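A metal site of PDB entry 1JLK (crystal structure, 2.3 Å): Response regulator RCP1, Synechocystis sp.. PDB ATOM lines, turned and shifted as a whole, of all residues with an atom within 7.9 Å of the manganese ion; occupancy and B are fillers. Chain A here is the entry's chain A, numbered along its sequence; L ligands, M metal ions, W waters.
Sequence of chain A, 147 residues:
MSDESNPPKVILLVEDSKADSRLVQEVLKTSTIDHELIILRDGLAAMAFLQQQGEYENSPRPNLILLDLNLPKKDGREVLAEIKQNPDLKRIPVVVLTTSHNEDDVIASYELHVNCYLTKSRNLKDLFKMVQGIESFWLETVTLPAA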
ATOM      1  N   VAL A  14     -25.223   2.173   5.856  1.00  0.00           N
ATOM      2  CA  VAL A  14     -23.937   2.573   5.311  1.00  0.00           C
ATOM      3  C   VAL A  14     -23.640   3.930   5.936  1.00  0.00           C
ATOM      4  O   VAL A  14     -24.128   4.959   5.464  1.00  0.00           O
ATOM      5  CB  VAL A  14     -24.003   2.698   3.784  1.00  0.00           C
ATOM      6  CG1 VAL A  14     -22.599   2.854   3.214  1.00  0.00           C
ATOM      7  CG2 VAL A  14     -24.665   1.469   3.192  1.00  0.00           C
ATOM      8  N   GLU A  15     -22.838   3.930   6.990  1.00  0.00           N
ATOM      9  CA  GLU A  15     -22.520   5.152   7.719  1.00  0.00           C
ATOM     10  C   GLU A  15     -21.096   5.133   8.281  1.00  0.00           C
ATOM     11  O   GLU A  15     -20.718   4.196   8.981  1.00  0.00           O
ATOM     12  CB  GLU A  15     -23.539   5.302   8.852  1.00  0.00           C
ATOM     13  CG  GLU A  15     -23.218   6.406   9.834  1.00  0.00           C
ATOM     14  CD  GLU A  15     -23.157   7.754   9.178  1.00  0.00           C
ATOM     15  OE1 GLU A  15     -24.179   8.182   8.593  1.00  0.00           O
ATOM     16  OE2 GLU A  15     -22.086   8.392   9.240  1.00  0.00           O
ATOM     17  N   ASP A  16     -20.314   6.172   7.991  1.00  0.00           N
ATOM     18  CA  ASP A  16     -18.935   6.258   8.467  1.00  0.00           C
ATOM     19  C   ASP A  16     -18.762   6.793   9.884  1.00  0.00           C
ATOM     20  O   ASP A  16     -17.740   6.558  10.516  1.00  0.00           O
ATOM     21  CB  ASP A  16     -18.073   7.079   7.503  1.00  0.00           C
ATOM     22  CG  ASP A  16     -18.677   8.427   7.158  1.00  0.00           C
ATOM     23  OD1 ASP A  16     -19.777   8.448   6.586  1.00  0.00           O
ATOM     24  OD2 ASP A  16     -18.051   9.470   7.460  1.00  0.00           O
ATOM     25  N   SER A  17     -19.744   7.516  10.395  1.00  0.00           N
ATOM     26  CA  SER A  17     -19.647   8.043  11.750  1.00  0.00           C
ATOM     27  C   SER A  17     -20.055   6.959  12.727  1.00  0.00           C
ATOM     28  O   SER A  17     -21.206   6.534  12.735  1.00  0.00           O
ATOM     29  CB  SER A  17     -20.560   9.261  11.925  1.00  0.00           C
ATOM     30  OG  SER A  17     -20.597   9.673  13.280  1.00  0.00           O
ATOM     31  N   ASP A  20     -23.162   8.297  14.937  1.00  0.00           N
ATOM     32  CA  ASP A  20     -24.449   8.173  14.248  1.00  0.00           C
ATOM     33  C   ASP A  20     -24.755   6.694  14.045  1.00  0.00           C
ATOM     34  O   ASP A  20     -25.908   6.246  14.159  1.00  0.00           O
ATOM     35  CB  ASP A  20     -24.390   8.881  12.887  1.00  0.00           C
ATOM     36  CG  ASP A  20     -24.092  10.371  13.019  1.00  0.00           C
ATOM     37  OD1 ASP A  20     -24.170  10.876  14.147  1.00  0.00           O
ATOM     38  OD2 ASP A  20     -23.800  11.015  11.986  1.00  0.00           O
ATOM     39  N   ARG A  41     -19.023   0.842   6.697  1.00  0.00           N
ATOM     40  CA  ARG A  41     -18.320   2.122   6.875  1.00  0.00           C
ATOM     41  C   ARG A  41     -17.939   2.970   5.670  1.00  0.00           C
ATOM     42  O   ARG A  41     -17.374   4.046   5.833  1.00  0.00           O
ATOM     43  CB  ARG A  41     -17.053   1.886   7.710  1.00  0.00           C
ATOM     44  CG  ARG A  41     -17.333   1.252   9.063  1.00  0.00           C
ATOM     45  CD  ARG A  41     -18.330   2.066   9.824  1.00  0.00           C
ATOM     46  NE  ARG A  41     -18.643   1.518  11.141  1.00  0.00           N
ATOM     47  CZ  ARG A  41     -19.504   2.100  11.970  1.00  0.00           C
ATOM     48  NH1 ARG A  41     -20.103   3.228  11.606  1.00  0.00           N
ATOM     49  NH2 ARG A  41     -19.759   1.570  13.164  1.00  0.00           N
ATOM     50  N   ASP A  68     -25.747   7.128   4.056  1.00  0.00           N
ATOM     51  CA  ASP A  68     -25.177   8.435   4.346  1.00  0.00           C
ATOM     52  C   ASP A  68     -24.468   8.776   3.039  1.00  0.00           C
ATOM     53  O   ASP A  68     -23.882   7.897   2.416  1.00  0.00           O
ATOM     54  CB  ASP A  68     -24.156   8.345   5.478  1.00  0.00           C
ATOM     55  CG  ASP A  68     -23.206   9.515   5.467  1.00  0.00           C
ATOM     56  OD1 ASP A  68     -23.669  10.675   5.490  1.00  0.00           O
ATOM     57  OD2 ASP A  68     -21.988   9.266   5.432  1.00  0.00           O
ATOM     58  N   LEU A  69     -24.534  10.027   2.612  1.00  0.00           N
ATOM     59  CA  LEU A  69     -23.911  10.401   1.343  1.00  0.00           C
ATOM     60  C   LEU A  69     -22.407  10.688   1.365  1.00  0.00           C
ATOM     61  O   LEU A  69     -21.667  10.203   0.501  1.00  0.00           O
ATOM     62  CB  LEU A  69     -24.648  11.600   0.736  1.00  0.00           C
ATOM     63  CG  LEU A  69     -26.119  11.368   0.377  1.00  0.00           C
ATOM     64  CD1 LEU A  69     -26.708  12.632  -0.224  1.00  0.00           C
ATOM     65  CD2 LEU A  69     -26.235  10.207  -0.605  1.00  0.00           C
ATOM     66  N   ASN A  70     -21.967  11.466   2.340  1.00  0.00           N
ATOM     67  CA  ASN A  70     -20.549  11.838   2.450  1.00  0.00           C
ATOM     68  C   ASN A  70     -19.772  10.673   3.082  1.00  0.00           C
ATOM     69  O   ASN A  70     -19.514  10.666   4.286  1.00  0.00           O
ATOM     70  CB  ASN A  70     -20.426  13.119   3.294  1.00  0.00           C
ATOM     71  CG  ASN A  70     -19.069  13.806   3.145  1.00  0.00           C
ATOM     72  OD1 ASN A  70     -18.014  13.198   3.344  1.00  0.00           O
ATOM     73  ND2 ASN A  70     -19.099  15.089   2.800  1.00  0.00           N
ATOM     74  N   LEU A  71     -19.412   9.699   2.255  1.00  0.00           N
ATOM     75  CA  LEU A  71     -18.676   8.515   2.692  1.00  0.00           C
ATOM     76  C   LEU A  71     -17.302   8.411   2.027  1.00  0.00           C
ATOM     77  O   LEU A  71     -17.092   8.957   0.943  1.00  0.00           O
ATOM     78  CB  LEU A  71     -19.443   7.253   2.346  1.00  0.00           C
ATOM     79  CG  LEU A  71     -20.850   7.009   2.885  1.00  0.00           C
ATOM     80  CD1 LEU A  71     -21.427   5.812   2.166  1.00  0.00           C
ATOM     81  CD2 LEU A  71     -20.794   6.755   4.387  1.00  0.00           C
ATOM     82  N   PRO A  72     -16.364   7.686   2.661  1.00  0.00           N
ATOM     83  CA  PRO A  72     -15.037   7.545   2.070  1.00  0.00           C
ATOM     84  C   PRO A  72     -15.066   6.477   0.977  1.00  0.00           C
ATOM     85  O   PRO A  72     -16.047   5.727   0.855  1.00  0.00           O
ATOM     86  CB  PRO A  72     -14.177   7.105   3.259  1.00  0.00           C
ATOM     87  CG  PRO A  72     -14.964   7.575   4.474  1.00  0.00           C
ATOM     88  CD  PRO A  72     -16.366   7.231   4.061  1.00  0.00           C
ATOM     89  N   LEU A  97     -29.884   9.278   4.543  1.00  0.00           N
ATOM     90  CA  LEU A  97     -29.875   9.852   5.892  1.00  0.00           C
ATOM     91  C   LEU A  97     -28.481  10.431   6.055  1.00  0.00           C
ATOM     92  O   LEU A  97     -27.563   9.730   6.475  1.00  0.00           O
ATOM     93  CB  LEU A  97     -30.121   8.772   6.938  1.00  0.00           C
ATOM     94  CG  LEU A  97     -30.207   9.288   8.377  1.00  0.00           C
ATOM     95  CD1 LEU A  97     -31.160  10.465   8.434  1.00  0.00           C
ATOM     96  CD2 LEU A  97     -30.653   8.171   9.315  1.00  0.00           C
ATOM     97  N   THR A  98     -28.338  11.700   5.701  1.00  0.00           N
ATOM     98  CA  THR A  98     -27.033  12.326   5.759  1.00  0.00           C
ATOM     99  C   THR A  98     -27.017  13.650   6.482  1.00  0.00           C
ATOM    100  O   THR A  98     -28.062  14.163   6.884  1.00  0.00           O
ATOM    101  CB  THR A  98     -26.479  12.547   4.353  1.00  0.00           C
ATOM    102  OG1 THR A  98     -25.097  12.908   4.445  1.00  0.00           O
ATOM    103  CG2 THR A  98     -27.243  13.657   3.649  1.00  0.00           C
ATOM    104  N   THR A  99     -25.829  14.226   6.616  1.00  0.00           N
ATOM    105  CA  THR A  99     -25.657  15.492   7.307  1.00  0.00           C
ATOM    106  C   THR A  99     -26.131  16.711   6.493  1.00  0.00           C
ATOM    107  O   THR A  99     -26.907  17.519   7.001  1.00  0.00           O
ATOM    108  CB  THR A  99     -24.178  15.675   7.743  1.00  0.00           C
ATOM    109  OG1 THR A  99     -24.139  16.310   9.017  1.00  0.00           O
ATOM    110  CG2 THR A  99     -23.399  16.538   6.738  1.00  0.00           C
ATOM    111  N   LYS A 120     -29.951  14.611   8.838  1.00  0.00           N
ATOM    112  CA  LYS A 120     -29.684  14.340  10.249  1.00  0.00           C
ATOM    113  C   LYS A 120     -29.840  15.619  11.050  1.00  0.00           C
ATOM    114  O   LYS A 120     -29.136  16.598  10.788  1.00  0.00           O
ATOM    115  CB  LYS A 120     -28.256  13.821  10.429  1.00  0.00           C
ATOM    116  CG  LYS A 120     -27.984  12.495   9.784  1.00  0.00           C
ATOM    117  CD  LYS A 120     -26.543  12.120  10.033  1.00  0.00           C
ATOM    118  CE  LYS A 120     -26.251  10.718   9.551  1.00  0.00           C
ATOM    119  NZ  LYS A 120     -24.829  10.367   9.827  1.00  0.00           N
HETATM  120  S1  LIG L   1     -20.597  13.676   7.367  1.00  0.00           S
HETATM  121  O1  LIG L   1     -21.471  12.982   6.396  1.00  0.00           O
HETATM  122  O2  LIG L   1     -19.622  12.711   7.913  1.00  0.00           O
HETATM  123  O3  LIG L   1     -19.874  14.773   6.691  1.00  0.00           O
HETATM  124  O4  LIG L   1     -21.416  14.218   8.461  1.00  0.00           O
HETATM  125 MN    MN M   1     -20.456  10.577   6.476  1.00  0.00          MN
HETATM  126  O   HOH W   1     -21.268  10.602   8.465  1.00  0.00           O
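OD1 of Asp 68 is in hydrogen-bond range of OG1 of Thr 98, 2.8 Å away. N of Asp 68 sits at hydrogen-bond distance from O of Val 14, at 3.1 Å. OE2 of Glu 15 is in hydrogen-bond range of N of Ser 17 (2.8 Å). NH1 of Arg 41 lies within hydrogen-bond range of O of Glu 15. The side-chain carboxylate of Glu 15 lies within salt-bridge range of the side-chain amino group of Lys 120 (2.6 Å).
Water W1 binds the manganese ion, at 2.1 Å. OD1 of Asp 16 binds the manganese ion. OD2 of Asp 68 binds the manganese ion (2.3 Å). The manganese ion is bound by the backbone carbonyl oxygen (O) of Asn 70. An oxygen (O1) of the ligand binds the manganese ion (2.6 Å). The manganese ion has five donor atoms within binding distance. Slightly farther from the manganese ion lies O2 of the ligand (2.7 Å). Slightly farther from the manganese ion lies OD2 of Asp 16 (2.8 Å).
OE2 of Glu 15 touches the manganese ion, at 3.9 Å. Four residues have an atom within 4 Å of the manganese ion: Glu 15, Asp 16, Asp 68 and Asn 70.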
